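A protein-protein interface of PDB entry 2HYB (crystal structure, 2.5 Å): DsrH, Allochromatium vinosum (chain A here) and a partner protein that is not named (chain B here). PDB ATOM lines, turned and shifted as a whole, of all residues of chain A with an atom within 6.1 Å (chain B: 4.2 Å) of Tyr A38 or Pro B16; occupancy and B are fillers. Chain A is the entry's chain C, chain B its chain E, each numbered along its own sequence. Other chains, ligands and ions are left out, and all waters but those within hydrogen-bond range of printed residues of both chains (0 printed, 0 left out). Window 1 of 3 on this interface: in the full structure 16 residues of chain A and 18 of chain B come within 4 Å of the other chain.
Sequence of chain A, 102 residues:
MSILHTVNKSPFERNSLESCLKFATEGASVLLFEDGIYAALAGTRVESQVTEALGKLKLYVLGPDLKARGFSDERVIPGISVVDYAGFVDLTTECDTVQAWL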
ATOM      1  N   SER A  10      -5.864   5.771 -13.277  1.00  0.00           N
ATOM      2  CA  SER A  10      -4.457   6.029 -13.619  1.00  0.00           C
ATOM      3  C   SER A  10      -3.508   5.749 -12.474  1.00  0.00           C
ATOM      4  O   SER A  10      -3.689   6.257 -11.375  1.00  0.00           O
ATOM      5  CB  SER A  10      -4.263   7.480 -14.069  1.00  0.00           C
ATOM      6  OG  SER A  10      -2.888   7.772 -14.235  1.00  0.00           O
ATOM      7  N   PRO A  11      -2.445   4.976 -12.731  1.00  0.00           N
ATOM      8  CA  PRO A  11      -1.501   4.665 -11.661  1.00  0.00           C
ATOM      9  C   PRO A  11      -0.717   5.884 -11.176  1.00  0.00           C
ATOM     10  O   PRO A  11      -0.008   5.808 -10.169  1.00  0.00           O
ATOM     11  CB  PRO A  11      -0.604   3.620 -12.300  1.00  0.00           C
ATOM     12  CG  PRO A  11      -0.476   4.143 -13.690  1.00  0.00           C
ATOM     13  CD  PRO A  11      -1.897   4.572 -14.039  1.00  0.00           C
ATOM     14  N   PHE A  12      -0.849   7.006 -11.883  1.00  0.00           N
ATOM     15  CA  PHE A  12      -0.129   8.222 -11.506  1.00  0.00           C
ATOM     16  C   PHE A  12      -1.005   9.160 -10.691  1.00  0.00           C
ATOM     17  O   PHE A  12      -0.547  10.180 -10.172  1.00  0.00           O
ATOM     18  CB  PHE A  12       0.390   8.932 -12.761  1.00  0.00           C
ATOM     19  CG  PHE A  12       1.030   8.005 -13.741  1.00  0.00           C
ATOM     20  CD1 PHE A  12       0.378   7.657 -14.923  1.00  0.00           C
ATOM     21  CD2 PHE A  12       2.254   7.417 -13.453  1.00  0.00           C
ATOM     22  CE1 PHE A  12       0.941   6.727 -15.807  1.00  0.00           C
ATOM     23  CE2 PHE A  12       2.833   6.483 -14.327  1.00  0.00           C
ATOM     24  CZ  PHE A  12       2.174   6.137 -15.503  1.00  0.00           C
ATOM     25  N   LEU A  32      -6.887  -3.786 -17.114  1.00  0.00           N
ATOM     26  CA  LEU A  32      -6.732  -2.340 -17.036  1.00  0.00           C
ATOM     27  C   LEU A  32      -7.628  -1.672 -18.081  1.00  0.00           C
ATOM     28  O   LEU A  32      -7.460  -1.897 -19.276  1.00  0.00           O
ATOM     29  CB  LEU A  32      -5.271  -1.955 -17.295  1.00  0.00           C
ATOM     30  CG  LEU A  32      -4.223  -2.490 -16.321  1.00  0.00           C
ATOM     31  CD1 LEU A  32      -2.823  -2.191 -16.843  1.00  0.00           C
ATOM     32  CD2 LEU A  32      -4.442  -1.863 -14.953  1.00  0.00           C
ATOM     33  N   GLU A  34     -10.453   2.031 -18.919  1.00  0.00           N
ATOM     34  CA  GLU A  34     -10.685   3.446 -18.610  1.00  0.00           C
ATOM     35  C   GLU A  34      -9.311   4.077 -18.344  1.00  0.00           C
ATOM     36  O   GLU A  34      -8.336   3.691 -18.976  1.00  0.00           O
ATOM     37  CB  GLU A  34     -11.629   3.601 -17.418  1.00  0.00           C
ATOM     38  CG  GLU A  34     -13.098   3.428 -17.817  1.00  0.00           C
ATOM     39  CD  GLU A  34     -14.079   3.666 -16.674  1.00  0.00           C
ATOM     40  OE1 GLU A  34     -13.696   4.324 -15.680  1.00  0.00           O
ATOM     41  OE2 GLU A  34     -15.243   3.214 -16.786  1.00  0.00           O
ATOM     42  N   ASP A  35      -9.203   5.032 -17.432  1.00  0.00           N
ATOM     43  CA  ASP A  35      -7.901   5.644 -17.186  1.00  0.00           C
ATOM     44  C   ASP A  35      -6.843   4.644 -16.686  1.00  0.00           C
ATOM     45  O   ASP A  35      -5.652   4.968 -16.605  1.00  0.00           O
ATOM     46  CB  ASP A  35      -8.054   6.822 -16.213  1.00  0.00           C
ATOM     47  CG  ASP A  35      -8.810   7.989 -16.833  1.00  0.00           C
ATOM     48  OD1 ASP A  35      -9.098   8.987 -16.130  1.00  0.00           O
ATOM     49  OD2 ASP A  35      -9.112   7.896 -18.038  1.00  0.00           O
ATOM     50  N   GLY A  36      -7.268   3.421 -16.376  1.00  0.00           N
ATOM     51  CA  GLY A  36      -6.323   2.421 -15.905  1.00  0.00           C
ATOM     52  C   GLY A  36      -5.294   2.053 -16.964  1.00  0.00           C
ATOM     53  O   GLY A  36      -4.185   1.618 -16.659  1.00  0.00           O
ATOM     54  N   ILE A  37      -5.684   2.245 -18.218  1.00  0.00           N
ATOM     55  CA  ILE A  37      -4.867   1.949 -19.384  1.00  0.00           C
ATOM     56  C   ILE A  37      -3.410   2.426 -19.338  1.00  0.00           C
ATOM     57  O   ILE A  37      -2.500   1.686 -19.697  1.00  0.00           O
ATOM     58  CB  ILE A  37      -5.577   2.514 -20.656  1.00  0.00           C
ATOM     59  CG1 ILE A  37      -6.025   1.347 -21.514  1.00  0.00           C
ATOM     60  CG2 ILE A  37      -4.692   3.501 -21.426  1.00  0.00           C
ATOM     61  CD1 ILE A  37      -7.041   0.491 -20.841  1.00  0.00           C
ATOM     62  N   TYR A  38      -3.187   3.653 -18.896  1.00  0.00           N
ATOM     63  CA  TYR A  38      -1.834   4.173 -18.863  1.00  0.00           C
ATOM     64  C   TYR A  38      -0.786   3.271 -18.182  1.00  0.00           C
ATOM     65  O   TYR A  38       0.412   3.372 -18.458  1.00  0.00           O
ATOM     66  CB  TYR A  38      -1.855   5.563 -18.243  1.00  0.00           C
ATOM     67  CG  TYR A  38      -2.760   6.514 -18.992  1.00  0.00           C
ATOM     68  CD1 TYR A  38      -3.884   7.051 -18.380  1.00  0.00           C
ATOM     69  CD2 TYR A  38      -2.469   6.912 -20.307  1.00  0.00           C
ATOM     70  CE1 TYR A  38      -4.698   7.968 -19.049  1.00  0.00           C
ATOM     71  CE2 TYR A  38      -3.270   7.829 -20.981  1.00  0.00           C
ATOM     72  CZ  TYR A  38      -4.386   8.360 -20.342  1.00  0.00           C
ATOM     73  OH  TYR A  38      -5.168   9.320 -20.946  1.00  0.00           O
ATOM     74  N   ALA A  39      -1.227   2.373 -17.311  1.00  0.00           N
ATOM     75  CA  ALA A  39      -0.290   1.479 -16.631  1.00  0.00           C
ATOM     76  C   ALA A  39       0.245   0.360 -17.531  1.00  0.00           C
ATOM     77  O   ALA A  39       1.265  -0.243 -17.217  1.00  0.00           O
ATOM     78  CB  ALA A  39      -0.947   0.878 -15.392  1.00  0.00           C
ATOM     79  N   ALA A  40      -0.435   0.081 -18.644  1.00  0.00           N
ATOM     80  CA  ALA A  40       0.008  -0.970 -19.565  1.00  0.00           C
ATOM     81  C   ALA A  40       0.967  -0.438 -20.623  1.00  0.00           C
ATOM     82  O   ALA A  40       1.434  -1.194 -21.466  1.00  0.00           O
ATOM     83  CB  ALA A  40      -1.189  -1.625 -20.250  1.00  0.00           C
ATOM     84  N   LEU A  41       1.259   0.859 -20.569  1.00  0.00           N
ATOM     85  CA  LEU A  41       2.153   1.496 -21.529  1.00  0.00           C
ATOM     86  C   LEU A  41       3.628   1.336 -21.184  1.00  0.00           C
ATOM     87  O   LEU A  41       4.044   1.572 -20.054  1.00  0.00           O
ATOM     88  CB  LEU A  41       1.821   2.989 -21.646  1.00  0.00           C
ATOM     89  CG  LEU A  41       0.418   3.294 -22.179  1.00  0.00           C
ATOM     90  CD1 LEU A  41       0.195   4.803 -22.243  1.00  0.00           C
ATOM     91  CD2 LEU A  41       0.260   2.648 -23.566  1.00  0.00           C
ATOM     92  N   ALA A  42       4.420   0.930 -22.165  1.00  0.00           N
ATOM     93  CA  ALA A  42       5.852   0.771 -21.956  1.00  0.00           C
ATOM     94  C   ALA A  42       6.479   2.142 -21.695  1.00  0.00           C
ATOM     95  O   ALA A  42       5.993   3.151 -22.202  1.00  0.00           O
ATOM     96  CB  ALA A  42       6.486   0.145 -23.192  1.00  0.00           C
ATOM     97  N   THR A  44       6.668   4.107 -18.863  1.00  0.00           N
ATOM     98  CA  THR A  44       6.290   4.891 -17.690  1.00  0.00           C
ATOM     99  C   THR A  44       7.012   4.488 -16.416  1.00  0.00           C
ATOM    100  O   THR A  44       7.632   3.430 -16.325  1.00  0.00           O
ATOM    101  CB  THR A  44       4.781   4.806 -17.370  1.00  0.00           C
ATOM    102  OG1 THR A  44       4.530   3.639 -16.581  1.00  0.00           O
ATOM    103  CG2 THR A  44       3.953   4.745 -18.648  1.00  0.00           C
ATOM    104  N   VAL A  46       5.983   3.281 -13.849  1.00  0.00           N
ATOM    105  CA  VAL A  46       5.551   2.005 -13.291  1.00  0.00           C
ATOM    106  C   VAL A  46       5.682   0.770 -14.179  1.00  0.00           C
ATOM    107  O   VAL A  46       5.082  -0.270 -13.908  1.00  0.00           O
ATOM    108  CB  VAL A  46       4.087   2.109 -12.795  1.00  0.00           C
ATOM    109  CG1 VAL A  46       3.945   3.318 -11.881  1.00  0.00           C
ATOM    110  CG2 VAL A  46       3.121   2.213 -13.970  1.00  0.00           C
ATOM    111  N   LEU A  66      -7.319   2.155 -24.879  1.00  0.00           N
ATOM    112  CA  LEU A  66      -5.936   2.458 -25.211  1.00  0.00           C
ATOM    113  C   LEU A  66      -5.970   3.398 -26.410  1.00  0.00           C
ATOM    114  O   LEU A  66      -5.319   4.443 -26.414  1.00  0.00           O
ATOM    115  CB  LEU A  66      -5.179   1.192 -25.599  1.00  0.00           C
ATOM    116  CG  LEU A  66      -4.371   0.473 -24.520  1.00  0.00           C
ATOM    117  CD1 LEU A  66      -3.810  -0.795 -25.119  1.00  0.00           C
ATOM    118  CD2 LEU A  66      -3.249   1.361 -23.997  1.00  0.00           C
ATOM    119  N   ALA A  68      -8.516   5.252 -27.638  1.00  0.00           N
ATOM    120  CA  ALA A  68      -9.161   6.524 -27.342  1.00  0.00           C
ATOM    121  C   ALA A  68      -8.176   7.506 -26.725  1.00  0.00           C
ATOM    122  O   ALA A  68      -8.289   8.721 -26.927  1.00  0.00           O
ATOM    123  CB  ALA A  68     -10.349   6.303 -26.401  1.00  0.00           C
ATOM    124  N   ARG A  69      -7.210   6.983 -25.972  1.00  0.00           N
ATOM    125  CA  ARG A  69      -6.226   7.847 -25.332  1.00  0.00           C
ATOM    126  C   ARG A  69      -4.983   8.097 -26.173  1.00  0.00           C
ATOM    127  O   ARG A  69      -4.071   8.822 -25.753  1.00  0.00           O
ATOM    128  CB  ARG A  69      -5.884   7.296 -23.943  1.00  0.00           C
ATOM    129  CG  ARG A  69      -7.094   7.400 -23.028  1.00  0.00           C
ATOM    130  CD  ARG A  69      -6.910   6.886 -21.617  1.00  0.00           C
ATOM    131  NE  ARG A  69      -8.154   7.036 -20.868  1.00  0.00           N
ATOM    132  CZ  ARG A  69      -9.273   6.360 -21.131  1.00  0.00           C
ATOM    133  NH1 ARG A  69      -9.309   5.477 -22.123  1.00  0.00           N
ATOM    134  NH2 ARG A  69     -10.367   6.576 -20.409  1.00  0.00           N
ATOM    135  N   PHE A  71      -3.015   5.449 -27.992  1.00  0.00           N
ATOM    136  CA  PHE A  71      -1.969   4.444 -27.992  1.00  0.00           C
ATOM    137  C   PHE A  71      -2.392   3.170 -28.672  1.00  0.00           C
ATOM    138  O   PHE A  71      -3.480   2.641 -28.431  1.00  0.00           O
ATOM    139  CB  PHE A  71      -1.516   4.112 -26.572  1.00  0.00           C
ATOM    140  CG  PHE A  71      -0.969   5.280 -25.827  1.00  0.00           C
ATOM    141  CD1 PHE A  71      -1.821   6.156 -25.168  1.00  0.00           C
ATOM    142  CD2 PHE A  71       0.398   5.521 -25.791  1.00  0.00           C
ATOM    143  CE1 PHE A  71      -1.320   7.260 -24.480  1.00  0.00           C
ATOM    144  CE2 PHE A  71       0.915   6.624 -25.105  1.00  0.00           C
ATOM    145  CZ  PHE A  71       0.054   7.495 -24.449  1.00  0.00           C
ATOM    146  N   LYS B  14      -5.862  16.139 -15.155  1.00  0.00           N
ATOM    147  CA  LYS B  14      -6.506  14.837 -15.275  1.00  0.00           C
ATOM    148  C   LYS B  14      -6.502  14.274 -16.685  1.00  0.00           C
ATOM    149  O   LYS B  14      -6.560  15.011 -17.661  1.00  0.00           O
ATOM    150  CB  LYS B  14      -7.947  14.925 -14.791  1.00  0.00           C
ATOM    151  CG  LYS B  14      -8.093  15.471 -13.390  1.00  0.00           C
ATOM    152  CD  LYS B  14      -9.559  15.706 -13.075  1.00  0.00           C
ATOM    153  CE  LYS B  14      -9.748  16.286 -11.690  1.00  0.00           C
ATOM    154  NZ  LYS B  14      -9.392  15.284 -10.659  1.00  0.00           N
ATOM    155  N   ALA B  15      -6.444  12.953 -16.782  1.00  0.00           N
ATOM    156  CA  ALA B  15      -6.459  12.272 -18.066  1.00  0.00           C
ATOM    157  C   ALA B  15      -7.812  12.498 -18.714  1.00  0.00           C
ATOM    158  O   ALA B  15      -8.801  12.689 -18.020  1.00  0.00           O
ATOM    159  CB  ALA B  15      -6.225  10.773 -17.857  1.00  0.00           C
ATOM    160  N   PRO B  16      -7.874  12.476 -20.055  1.00  0.00           N
ATOM    161  CA  PRO B  16      -9.138  12.678 -20.768  1.00  0.00           C
ATOM    162  C   PRO B  16     -10.003  11.417 -20.801  1.00  0.00           C
ATOM    163  O   PRO B  16      -9.525  10.318 -20.553  1.00  0.00           O
ATOM    164  CB  PRO B  16      -8.673  13.078 -22.164  1.00  0.00           C
ATOM    165  CG  PRO B  16      -7.456  12.238 -22.335  1.00  0.00           C
ATOM    166  CD  PRO B  16      -6.746  12.451 -21.005  1.00  0.00           C
ATOM    167  N   TYR B  17     -11.282  11.602 -21.107  1.00  0.00           N
ATOM    168  CA  TYR B  17     -12.261  10.520 -21.227  1.00  0.00           C
ATOM    169  C   TYR B  17     -12.602   9.724 -19.960  1.00  0.00           C
ATOM    170  O   TYR B  17     -13.749   9.287 -19.791  1.00  0.00           O
ATOM    171  CB  TYR B  17     -11.845   9.565 -22.356  1.00  0.00           C
ATOM    172  CG  TYR B  17     -11.559  10.273 -23.668  1.00  0.00           C
ATOM    173  CD1 TYR B  17     -10.256  10.648 -24.010  1.00  0.00           C
ATOM    174  CD2 TYR B  17     -12.592  10.606 -24.553  1.00  0.00           C
ATOM    175  CE1 TYR B  17      -9.989  11.337 -25.199  1.00  0.00           C
ATOM    176  CE2 TYR B  17     -12.333  11.291 -25.736  1.00  0.00           C
ATOM    177  CZ  TYR B  17     -11.028  11.655 -26.055  1.00  0.00           C
ATOM    178  OH  TYR B  17     -10.758  12.330 -27.223  1.00  0.00           O
ATOM    179  N   GLY B  18     -11.630   9.510 -19.080  1.00  0.00           N
ATOM    180  CA  GLY B  18     -11.934   8.800 -17.846  1.00  0.00           C
ATOM    181  C   GLY B  18     -12.971   9.653 -17.141  1.00  0.00           C
ATOM    182  O   GLY B  18     -13.915   9.153 -16.533  1.00  0.00           O
ATOM    183  N   ALA B  22     -11.401  17.101 -18.625  1.00  0.00           N
ATOM    184  CA  ALA B  22     -10.579  17.515 -19.761  1.00  0.00           C
ATOM    185  C   ALA B  22     -11.376  18.272 -20.822  1.00  0.00           C
ATOM    186  O   ALA B  22     -10.989  19.374 -21.242  1.00  0.00           O
ATOM    187  CB  ALA B  22      -9.900  16.291 -20.393  1.00  0.00           C
ATOM    188  N   TYR B  49      -1.667  13.990 -20.667  1.00  0.00           N
ATOM    189  CA  TYR B  49      -2.306  13.007 -21.525  1.00  0.00           C
ATOM    190  C   TYR B  49      -3.452  13.641 -22.301  1.00  0.00           C
ATOM    191  O   TYR B  49      -4.013  13.033 -23.217  1.00  0.00           O
ATOM    192  CB  TYR B  49      -2.812  11.846 -20.693  1.00  0.00           C
ATOM    193  CG  TYR B  49      -1.748  10.873 -20.262  1.00  0.00           C
ATOM    194  CD1 TYR B  49      -1.732  10.377 -18.952  1.00  0.00           C
ATOM    195  CD2 TYR B  49      -0.864  10.324 -21.186  1.00  0.00           C
ATOM    196  CE1 TYR B  49      -0.881   9.342 -18.574  1.00  0.00           C
ATOM    197  CE2 TYR B  49       0.000   9.284 -20.827  1.00  0.00           C
ATOM    198  CZ  TYR B  49      -0.022   8.786 -19.511  1.00  0.00           C
ATOM    199  OH  TYR B  49       0.734   7.680 -19.159  1.00  0.00           O
ATOM    200  N   GLN B  50      -3.805  14.867 -21.928  1.00  0.00           N
ATOM    201  CA  GLN B  50      -4.872  15.567 -22.623  1.00  0.00           C
ATOM    202  C   GLN B  50      -4.453  15.961 -24.042  1.00  0.00           C
ATOM    203  O   GLN B  50      -5.285  15.968 -24.945  1.00  0.00           O
ATOM    204  CB  GLN B  50      -5.303  16.810 -21.834  1.00  0.00           C
ATOM    205  CG  GLN B  50      -6.393  16.543 -20.799  1.00  0.00           C
ATOM    206  CD  GLN B  50      -6.767  17.782 -19.980  1.00  0.00           C
ATOM    207  OE1 GLN B  50      -6.871  18.887 -20.515  1.00  0.00           O
ATOM    208  NE2 GLN B  50      -6.989  17.594 -18.680  1.00  0.00           N
ATOM    209  N   PHE B  65     -12.822  14.708 -28.939  1.00  0.00           N
ATOM    210  CA  PHE B  65     -12.728  16.161 -28.916  1.00  0.00           C
ATOM    211  C   PHE B  65     -11.325  16.746 -29.025  1.00  0.00           C
ATOM    212  O   PHE B  65     -11.179  17.969 -29.004  1.00  0.00           O
ATOM    213  CB  PHE B  65     -13.369  16.710 -27.637  1.00  0.00           C
ATOM    214  CG  PHE B  65     -12.674  16.274 -26.366  1.00  0.00           C
ATOM    215  CD1 PHE B  65     -12.869  14.993 -25.848  1.00  0.00           C
ATOM    216  CD2 PHE B  65     -11.845  17.153 -25.674  1.00  0.00           C
ATOM    217  CE1 PHE B  65     -12.251  14.598 -24.662  1.00  0.00           C
ATOM    218  CE2 PHE B  65     -11.223  16.772 -24.491  1.00  0.00           C
ATOM    219  CZ  PHE B  65     -11.428  15.492 -23.980  1.00  0.00           C
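Among the printed residues, pairs that only touch across the chains: Tyr A38 with Tyr B49 (3.2 Å), Tyr A38 with Ala B15 (3.4 Å), Phe A12 with Tyr B49 (3.5 Å), Tyr A38 with Pro B16 (3.5 Å), Asp A35 with Pro B16 (3.5 Å), Ala A68 with Tyr B17 (3.6 Å), Arg A69 with Pro B16 (3.6 Å), Asp A35 with Ala B15 (3.8 Å) and Arg A69 with Tyr B17 (3.9 Å).
The side-chain carboxylate (OD2) of Asp A35 lies close to the backbone NH (N) of Gly B18, 3.2 Å away. The backbone NH (N) of Gly B18 sits close to the guanidinium group (NH2) of Arg A69, at 3.5 Å.
The side-chain hydroxyl of Ser A10 lies close to the backbone NH of Phe A12 (3.2 Å). N of Ser A10 sits close to O of Asp A35, at 3.4 Å. The side-chain carboxylate (OD2) of Asp A35 is in salt-bridge range of the guanidinium group (NH2) of Arg A69 (3.0 Å).
Hydrophobic or aromatic side chains of chain B within 4 Å of the printed part of chain A: Ala B15, Pro B16, Tyr B17 and Tyr B49. Hydrophobic or aromatic side chains of chain A that line the printed part of chain B: Phe A12 and Tyr A38. Along chain A the printed residues that touch a printed residue of chain B span positions 12 to 69. Among the printed residues, 11 pairs touch across the chains. Among the printed residues, no Asp or Glu carboxylate lies within 4 Å of a Lys or Arg side-chain nitrogen of the other chain.
Of chain B, only Ala B15, Pro B16 and Tyr B49 come within 4 Å of Tyr A38. Pro B16 touches just these residues of chain A: Asp A35, Tyr A38 and Arg A69. Of the printed residues of chain A, Tyr B49 touches Phe A12 and Tyr A38. Printed residues of chain B within 4 Å of Phe A12: Tyr B49 (3.5 Å). Printed residues of chain A within 4 Å of Ala B15: Asp A35 (3.8 Å) and Tyr A38 (3.4 Å). Of the printed residues of chain B, Asp A35 touches Ala B15 (3.8 Å), Pro B16 (3.5 Å) and Gly B18 (3.0 Å). The nearest residue of chain A that does not touch Pro B16 is Ala A68 (5.8 Å).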
